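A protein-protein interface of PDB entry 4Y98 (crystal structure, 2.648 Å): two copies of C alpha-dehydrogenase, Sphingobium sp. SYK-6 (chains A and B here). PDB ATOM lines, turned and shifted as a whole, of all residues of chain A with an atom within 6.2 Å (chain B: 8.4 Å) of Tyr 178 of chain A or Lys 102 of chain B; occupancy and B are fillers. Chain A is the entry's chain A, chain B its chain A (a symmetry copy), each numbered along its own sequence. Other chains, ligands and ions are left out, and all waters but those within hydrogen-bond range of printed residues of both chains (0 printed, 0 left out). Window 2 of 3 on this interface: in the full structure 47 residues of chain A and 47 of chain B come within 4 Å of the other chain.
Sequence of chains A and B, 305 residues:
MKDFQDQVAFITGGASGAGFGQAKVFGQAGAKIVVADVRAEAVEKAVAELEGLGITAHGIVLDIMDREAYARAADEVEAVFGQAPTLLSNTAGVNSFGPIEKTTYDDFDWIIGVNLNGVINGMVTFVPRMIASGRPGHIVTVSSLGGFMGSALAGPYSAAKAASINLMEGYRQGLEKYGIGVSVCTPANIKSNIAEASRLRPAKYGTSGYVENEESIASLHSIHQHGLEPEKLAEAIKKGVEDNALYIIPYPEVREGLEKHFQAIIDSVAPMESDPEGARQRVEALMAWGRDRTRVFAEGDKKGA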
ATOM      1  N   VAL A 127      -2.500  24.909  14.634  1.00  0.00           N
ATOM      2  CA  VAL A 127      -3.293  25.562  15.689  1.00  0.00           C
ATOM      3  C   VAL A 127      -2.640  26.845  16.222  1.00  0.00           C
ATOM      4  O   VAL A 127      -3.298  27.882  16.313  1.00  0.00           O
ATOM      5  CB  VAL A 127      -3.564  24.600  16.876  1.00  0.00           C
ATOM      6  CG1 VAL A 127      -4.062  25.360  18.109  1.00  0.00           C
ATOM      7  CG2 VAL A 127      -4.588  23.552  16.479  1.00  0.00           C
ATOM      8  N   ILE A 131      -4.102  30.640  15.554  1.00  0.00           N
ATOM      9  CA  ILE A 131      -4.398  31.495  16.689  1.00  0.00           C
ATOM     10  C   ILE A 131      -3.637  32.806  16.580  1.00  0.00           C
ATOM     11  O   ILE A 131      -4.187  33.874  16.837  1.00  0.00           O
ATOM     12  CB  ILE A 131      -4.052  30.785  18.009  1.00  0.00           C
ATOM     13  CG1 ILE A 131      -5.266  29.982  18.473  1.00  0.00           C
ATOM     14  CG2 ILE A 131      -3.625  31.782  19.095  1.00  0.00           C
ATOM     15  CD1 ILE A 131      -5.005  29.081  19.646  1.00  0.00           C
ATOM     16  N   GLY A 134      -4.941  35.632  14.427  1.00  0.00           N
ATOM     17  CA  GLY A 134      -5.987  36.452  15.003  1.00  0.00           C
ATOM     18  C   GLY A 134      -7.218  36.488  14.127  1.00  0.00           C
ATOM     19  O   GLY A 134      -8.088  37.333  14.308  1.00  0.00           O
ATOM     20  N   ARG A 135      -7.292  35.569  13.173  1.00  0.00           N
ATOM     21  CA  ARG A 135      -8.427  35.508  12.266  1.00  0.00           C
ATOM     22  C   ARG A 135      -9.362  34.390  12.692  1.00  0.00           C
ATOM     23  O   ARG A 135      -8.918  33.410  13.288  1.00  0.00           O
ATOM     24  CB  ARG A 135      -7.961  35.285  10.822  1.00  0.00           C
ATOM     25  CG  ARG A 135      -7.881  36.552   9.982  1.00  0.00           C
ATOM     26  CD  ARG A 135      -7.390  36.246   8.574  1.00  0.00           C
ATOM     27  NE  ARG A 135      -6.003  35.783   8.578  1.00  0.00           N
ATOM     28  CZ  ARG A 135      -4.950  36.530   8.248  1.00  0.00           C
ATOM     29  NH1 ARG A 135      -5.098  37.795   7.863  1.00  0.00           N
ATOM     30  NH2 ARG A 135      -3.735  36.003   8.297  1.00  0.00           N
ATOM     31  N   PRO A 136     -10.664  34.542  12.403  1.00  0.00           N
ATOM     32  CA  PRO A 136     -11.564  33.392  12.498  1.00  0.00           C
ATOM     33  C   PRO A 136     -11.062  32.261  11.627  1.00  0.00           C
ATOM     34  O   PRO A 136     -10.329  32.500  10.669  1.00  0.00           O
ATOM     35  CB  PRO A 136     -12.901  33.931  11.988  1.00  0.00           C
ATOM     36  CG  PRO A 136     -12.840  35.384  12.224  1.00  0.00           C
ATOM     37  CD  PRO A 136     -11.394  35.786  12.103  1.00  0.00           C
ATOM     38  N   GLY A 137     -11.439  31.042  11.965  1.00  0.00           N
ATOM     39  CA  GLY A 137     -10.978  29.890  11.226  1.00  0.00           C
ATOM     40  C   GLY A 137     -11.840  28.694  11.544  1.00  0.00           C
ATOM     41  O   GLY A 137     -12.834  28.816  12.263  1.00  0.00           O
ATOM     42  N   GLY A 174     -11.584  23.739  23.305  1.00  0.00           N
ATOM     43  CA  GLY A 174     -10.434  24.610  23.465  1.00  0.00           C
ATOM     44  C   GLY A 174     -10.480  25.857  22.596  1.00  0.00           C
ATOM     45  O   GLY A 174     -10.191  26.956  23.061  1.00  0.00           O
ATOM     46  N   LEU A 175     -10.862  25.698  21.337  1.00  0.00           N
ATOM     47  CA  LEU A 175     -10.632  26.748  20.356  1.00  0.00           C
ATOM     48  C   LEU A 175     -11.797  27.710  20.153  1.00  0.00           C
ATOM     49  O   LEU A 175     -11.654  28.714  19.459  1.00  0.00           O
ATOM     50  CB  LEU A 175     -10.267  26.112  19.022  1.00  0.00           C
ATOM     51  CG  LEU A 175      -8.980  25.296  19.098  1.00  0.00           C
ATOM     52  CD1 LEU A 175      -8.756  24.598  17.800  1.00  0.00           C
ATOM     53  CD2 LEU A 175      -7.776  26.166  19.428  1.00  0.00           C
ATOM     54  N   GLU A 176     -12.943  27.409  20.753  1.00  0.00           N
ATOM     55  CA  GLU A 176     -14.108  28.269  20.618  1.00  0.00           C
ATOM     56  C   GLU A 176     -13.797  29.679  21.066  1.00  0.00           C
ATOM     57  O   GLU A 176     -14.289  30.649  20.501  1.00  0.00           O
ATOM     58  CB  GLU A 176     -15.272  27.725  21.430  1.00  0.00           C
ATOM     59  CG  GLU A 176     -16.369  28.739  21.662  1.00  0.00           C
ATOM     60  CD  GLU A 176     -17.634  28.105  22.194  1.00  0.00           C
ATOM     61  OE1 GLU A 176     -18.087  27.106  21.596  1.00  0.00           O
ATOM     62  OE2 GLU A 176     -18.172  28.597  23.213  1.00  0.00           O
ATOM     63  N   LYS A 177     -12.976  29.789  22.096  1.00  0.00           N
ATOM     64  CA  LYS A 177     -12.631  31.095  22.624  1.00  0.00           C
ATOM     65  C   LYS A 177     -11.775  31.865  21.626  1.00  0.00           C
ATOM     66  O   LYS A 177     -11.567  33.064  21.784  1.00  0.00           O
ATOM     67  CB  LYS A 177     -11.913  30.966  23.972  1.00  0.00           C
ATOM     68  CG  LYS A 177     -10.778  29.927  24.042  1.00  0.00           C
ATOM     69  CD  LYS A 177     -10.095  29.951  25.431  1.00  0.00           C
ATOM     70  CE  LYS A 177      -8.930  28.970  25.570  1.00  0.00           C
ATOM     71  NZ  LYS A 177      -9.363  27.615  26.018  1.00  0.00           N
ATOM     72  N   TYR A 178     -11.292  31.179  20.594  1.00  0.00           N
ATOM     73  CA  TYR A 178     -10.468  31.825  19.578  1.00  0.00           C
ATOM     74  C   TYR A 178     -11.230  32.059  18.280  1.00  0.00           C
ATOM     75  O   TYR A 178     -10.637  32.414  17.263  1.00  0.00           O
ATOM     76  CB  TYR A 178      -9.223  30.991  19.296  1.00  0.00           C
ATOM     77  CG  TYR A 178      -8.345  30.853  20.501  1.00  0.00           C
ATOM     78  CD1 TYR A 178      -7.564  31.915  20.938  1.00  0.00           C
ATOM     79  CD2 TYR A 178      -8.307  29.668  21.215  1.00  0.00           C
ATOM     80  CE1 TYR A 178      -6.761  31.795  22.057  1.00  0.00           C
ATOM     81  CE2 TYR A 178      -7.509  29.536  22.331  1.00  0.00           C
ATOM     82  CZ  TYR A 178      -6.739  30.600  22.751  1.00  0.00           C
ATOM     83  OH  TYR A 178      -5.950  30.451  23.868  1.00  0.00           O
ATOM     84  N   GLY A 179     -12.543  31.865  18.319  1.00  0.00           N
ATOM     85  CA  GLY A 179     -13.362  32.029  17.138  1.00  0.00           C
ATOM     86  C   GLY A 179     -13.045  30.980  16.088  1.00  0.00           C
ATOM     87  O   GLY A 179     -13.378  31.141  14.911  1.00  0.00           O
ATOM     88  N   ILE A 180     -12.389  29.907  16.517  1.00  0.00           N
ATOM     89  CA  ILE A 180     -12.055  28.807  15.622  1.00  0.00           C
ATOM     90  C   ILE A 180     -12.944  27.621  15.936  1.00  0.00           C
ATOM     91  O   ILE A 180     -12.881  27.036  17.022  1.00  0.00           O
ATOM     92  CB  ILE A 180     -10.579  28.400  15.732  1.00  0.00           C
ATOM     93  CG1 ILE A 180      -9.689  29.617  15.476  1.00  0.00           C
ATOM     94  CG2 ILE A 180     -10.262  27.282  14.752  1.00  0.00           C
ATOM     95  CD1 ILE A 180      -8.203  29.358  15.630  1.00  0.00           C
ATOM     96  N   PHE B  97      -2.485  17.925  32.887  1.00  0.00           N
ATOM     97  CA  PHE B  97      -3.565  18.823  32.522  1.00  0.00           C
ATOM     98  C   PHE B  97      -2.993  20.067  31.880  1.00  0.00           C
ATOM     99  O   PHE B  97      -1.821  20.396  32.075  1.00  0.00           O
ATOM    100  CB  PHE B  97      -4.404  19.194  33.745  1.00  0.00           C
ATOM    101  CG  PHE B  97      -5.268  18.072  34.256  1.00  0.00           C
ATOM    102  CD1 PHE B  97      -6.445  17.735  33.609  1.00  0.00           C
ATOM    103  CD2 PHE B  97      -4.906  17.360  35.381  1.00  0.00           C
ATOM    104  CE1 PHE B  97      -7.241  16.708  34.071  1.00  0.00           C
ATOM    105  CE2 PHE B  97      -5.705  16.332  35.851  1.00  0.00           C
ATOM    106  CZ  PHE B  97      -6.872  16.009  35.192  1.00  0.00           C
ATOM    107  N   GLY B  98      -3.825  20.749  31.105  1.00  0.00           N
ATOM    108  CA  GLY B  98      -3.436  21.985  30.456  1.00  0.00           C
ATOM    109  C   GLY B  98      -4.254  22.203  29.202  1.00  0.00           C
ATOM    110  O   GLY B  98      -4.912  21.281  28.727  1.00  0.00           O
ATOM    111  N   PRO B  99      -4.225  23.427  28.661  1.00  0.00           N
ATOM    112  CA  PRO B  99      -5.067  23.729  27.506  1.00  0.00           C
ATOM    113  C   PRO B  99      -4.646  22.939  26.273  1.00  0.00           C
ATOM    114  O   PRO B  99      -3.459  22.893  25.933  1.00  0.00           O
ATOM    115  CB  PRO B  99      -4.858  25.234  27.290  1.00  0.00           C
ATOM    116  CG  PRO B  99      -4.210  25.736  28.484  1.00  0.00           C
ATOM    117  CD  PRO B  99      -3.433  24.593  29.068  1.00  0.00           C
ATOM    118  N   ILE B 100      -5.629  22.340  25.612  1.00  0.00           N
ATOM    119  CA  ILE B 100      -5.383  21.457  24.487  1.00  0.00           C
ATOM    120  C   ILE B 100      -4.621  22.164  23.357  1.00  0.00           C
ATOM    121  O   ILE B 100      -3.846  21.531  22.638  1.00  0.00           O
ATOM    122  CB  ILE B 100      -6.717  20.892  23.964  1.00  0.00           C
ATOM    123  CG1 ILE B 100      -6.466  19.692  23.050  1.00  0.00           C
ATOM    124  CG2 ILE B 100      -7.547  21.996  23.288  1.00  0.00           C
ATOM    125  CD1 ILE B 100      -7.751  18.967  22.630  1.00  0.00           C
ATOM    126  N   GLU B 101      -4.831  23.473  23.227  1.00  0.00           N
ATOM    127  CA  GLU B 101      -4.164  24.265  22.194  1.00  0.00           C
ATOM    128  C   GLU B 101      -2.673  24.317  22.423  1.00  0.00           C
ATOM    129  O   GLU B 101      -1.889  24.426  21.478  1.00  0.00           O
ATOM    130  CB  GLU B 101      -4.675  25.702  22.163  1.00  0.00           C
ATOM    131  CG  GLU B 101      -6.142  25.871  22.444  1.00  0.00           C
ATOM    132  CD  GLU B 101      -6.427  26.035  23.913  1.00  0.00           C
ATOM    133  OE1 GLU B 101      -6.897  25.053  24.511  1.00  0.00           O
ATOM    134  OE2 GLU B 101      -6.183  27.133  24.461  1.00  0.00           O
ATOM    135  N   LYS B 102      -2.299  24.294  23.698  1.00  0.00           N
ATOM    136  CA  LYS B 102      -0.910  24.466  24.116  1.00  0.00           C
ATOM    137  C   LYS B 102      -0.136  23.159  24.053  1.00  0.00           C
ATOM    138  O   LYS B 102       1.057  23.126  24.359  1.00  0.00           O
ATOM    139  CB  LYS B 102      -0.841  25.021  25.549  1.00  0.00           C
ATOM    140  CG  LYS B 102      -0.910  26.543  25.693  1.00  0.00           C
ATOM    141  CD  LYS B 102      -2.269  27.077  25.316  1.00  0.00           C
ATOM    142  CE  LYS B 102      -2.425  28.555  25.611  1.00  0.00           C
ATOM    143  NZ  LYS B 102      -3.699  29.061  25.030  1.00  0.00           N
ATOM    144  N   THR B 103      -0.812  22.083  23.667  1.00  0.00           N
ATOM    145  CA  THR B 103      -0.222  20.757  23.749  1.00  0.00           C
ATOM    146  C   THR B 103       0.965  20.654  22.817  1.00  0.00           C
ATOM    147  O   THR B 103       0.956  21.239  21.744  1.00  0.00           O
ATOM    148  CB  THR B 103      -1.241  19.673  23.407  1.00  0.00           C
ATOM    149  OG1 THR B 103      -2.389  19.819  24.250  1.00  0.00           O
ATOM    150  CG2 THR B 103      -0.641  18.294  23.602  1.00  0.00           C
ATOM    151  N   THR B 104       1.981  19.907  23.228  1.00  0.00           N
ATOM    152  CA  THR B 104       3.208  19.764  22.454  1.00  0.00           C
ATOM    153  C   THR B 104       3.393  18.331  22.004  1.00  0.00           C
ATOM    154  O   THR B 104       2.665  17.435  22.429  1.00  0.00           O
ATOM    155  CB  THR B 104       4.438  20.158  23.266  1.00  0.00           C
ATOM    156  OG1 THR B 104       4.716  19.120  24.215  1.00  0.00           O
ATOM    157  CG2 THR B 104       4.195  21.471  23.995  1.00  0.00           C
ATOM    158  N   TYR B 105       4.391  18.111  21.161  1.00  0.00           N
ATOM    159  CA  TYR B 105       4.660  16.781  20.656  1.00  0.00           C
ATOM    160  C   TYR B 105       5.051  15.854  21.805  1.00  0.00           C
ATOM    161  O   TYR B 105       4.604  14.709  21.866  1.00  0.00           O
ATOM    162  CB  TYR B 105       5.754  16.826  19.585  1.00  0.00           C
ATOM    163  CG  TYR B 105       5.256  17.239  18.211  1.00  0.00           C
ATOM    164  CD1 TYR B 105       4.122  16.660  17.657  1.00  0.00           C
ATOM    165  CD2 TYR B 105       5.919  18.207  17.470  1.00  0.00           C
ATOM    166  CE1 TYR B 105       3.663  17.028  16.407  1.00  0.00           C
ATOM    167  CE2 TYR B 105       5.462  18.584  16.213  1.00  0.00           C
ATOM    168  CZ  TYR B 105       4.332  17.989  15.688  1.00  0.00           C
ATOM    169  OH  TYR B 105       3.859  18.347  14.441  1.00  0.00           O
ATOM    170  N   ASP B 107       4.239  16.201  25.000  1.00  0.00           N
ATOM    171  CA  ASP B 107       2.992  15.922  25.699  1.00  0.00           C
ATOM    172  C   ASP B 107       2.298  14.737  25.040  1.00  0.00           C
ATOM    173  O   ASP B 107       1.934  13.772  25.714  1.00  0.00           O
ATOM    174  CB  ASP B 107       2.053  17.125  25.679  1.00  0.00           C
ATOM    175  CG  ASP B 107       2.566  18.288  26.491  1.00  0.00           C
ATOM    176  OD1 ASP B 107       3.676  18.183  27.054  1.00  0.00           O
ATOM    177  OD2 ASP B 107       1.854  19.317  26.553  1.00  0.00           O
ATOM    178  N   PHE B 108       2.122  14.821  23.716  1.00  0.00           N
ATOM    179  CA  PHE B 108       1.417  13.779  22.982  1.00  0.00           C
ATOM    180  C   PHE B 108       2.125  12.447  23.077  1.00  0.00           C
ATOM    181  O   PHE B 108       1.519  11.448  23.453  1.00  0.00           O
ATOM    182  CB  PHE B 108       1.254  14.149  21.509  1.00  0.00           C
ATOM    183  CG  PHE B 108       0.044  14.987  21.231  1.00  0.00           C
ATOM    184  CD1 PHE B 108      -1.226  14.442  21.286  1.00  0.00           C
ATOM    185  CD2 PHE B 108       0.177  16.325  20.932  1.00  0.00           C
ATOM    186  CE1 PHE B 108      -2.338  15.221  21.043  1.00  0.00           C
ATOM    187  CE2 PHE B 108      -0.929  17.105  20.683  1.00  0.00           C
ATOM    188  CZ  PHE B 108      -2.190  16.553  20.741  1.00  0.00           C
ATOM    189  N   ALA B 152     -11.076  19.784  26.861  1.00  0.00           N
ATOM    190  CA  ALA B 152     -10.118  20.831  26.561  1.00  0.00           C
ATOM    191  C   ALA B 152      -8.878  20.766  27.447  1.00  0.00           C
ATOM    192  O   ALA B 152      -7.815  21.245  27.046  1.00  0.00           O
ATOM    193  CB  ALA B 152     -10.777  22.188  26.691  1.00  0.00           C
ATOM    194  N   PRO B 156      -5.280  15.089  25.026  1.00  0.00           N
ATOM    195  CA  PRO B 156      -4.475  13.943  24.586  1.00  0.00           C
ATOM    196  C   PRO B 156      -4.887  12.676  25.311  1.00  0.00           C
ATOM    197  O   PRO B 156      -5.122  11.649  24.667  1.00  0.00           O
ATOM    198  CB  PRO B 156      -3.041  14.341  24.954  1.00  0.00           C
ATOM    199  CG  PRO B 156      -3.062  15.821  25.053  1.00  0.00           C
ATOM    200  CD  PRO B 156      -4.441  16.193  25.525  1.00  0.00           C
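Tyr 178 of chain A touches just these residues of chain B: Glu 101 and Lys 102.
Lys 102 of chain B touches just one residue of chain A: Tyr 178 (2.9 Å).
Gly 179 of chain A touches none of the printed residues of chain B.
Of the printed residues of chain B, Lys 177 of chain A touches Glu 101.
Printed residues of chain A within 4 Å of Ile 100 of chain B: Gly 174 (3.9 Å).
Printed residues of chain A within 4 Å of Ala 152 of chain B: Gly 174 (3.8 Å).
Printed residues of chain A within 4 Å of Glu 101 of chain B: Gly 174, Leu 175, Lys 177 and Tyr 178.
Val 127 of chain A touches none of the printed residues of chain B.
Ile 180 of chain A touches none of the printed residues of chain B.
The nearest residue of chain B that does not touch Tyr 178 of chain A is Pro 99 of chain B (6.3 Å).
The nearest residue of chain A that does not touch Lys 102 of chain B is Lys 177 of chain A (5.3 Å).
No position is printed for both chains.
OE2 of Glu 101 of chain B is in salt-bridge range of NZ of Lys 177 of chain A, 3.6 Å away.
The side-chain hydroxyl of Tyr 178 of chain A sits at hydrogen-bond distance from the side-chain carboxylate of Glu 101 of chain B (3.4 Å).
OH of Tyr 178 of chain A is in hydrogen-bond range of NZ of Lys 102 of chain B (2.9 Å).
Hydrophobic or aromatic side chains of chain B within 4 Å of the printed part of chain A: Ile 100 and Ala 152.
Printed residues of chain A that touch a printed residue of chain B: Gly 174, Leu 175, Lys 177 and Tyr 178.
Hydrophobic or aromatic side chains of chain A that line the printed part of chain B: Leu 175 and Tyr 178.
The backbone carbonyl oxygen (O) of Gly 174 of chain A lies within hydrogen-bond range of the side-chain amino group (NZ) of Lys 177 of chain A, 3.1 Å away.
The backbone carbonyl oxygen (O) of Leu 175 of chain A is in hydrogen-bond range of the backbone NH (N) of Ile 180 of chain A (3.3 Å).
The side-chain hydroxyl of Thr 103 of chain B sits at hydrogen-bond distance from the backbone carbonyl oxygen of Ile 100 of chain B (2.8 Å).
The backbone NH (N) of Ile 100 of chain B is in hydrogen-bond range of the backbone carbonyl oxygen (O) of Ala 152 of chain B (2.8 Å).
NZ of Lys 102 of chain B is in salt-bridge range of OE2 of Glu 101 of chain B (3.2 Å).
Among the printed residues, pairs that only touch across the chains: Gly 174 of chain A with Ile 100 of chain B (3.9 Å), Gly 174 of chain A with Glu 101 of chain B (3.7 Å), Gly 174 of chain A with Ala 152 of chain B (3.8 Å) and Leu 175 of chain A with Glu 101 of chain B (3.4 Å).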
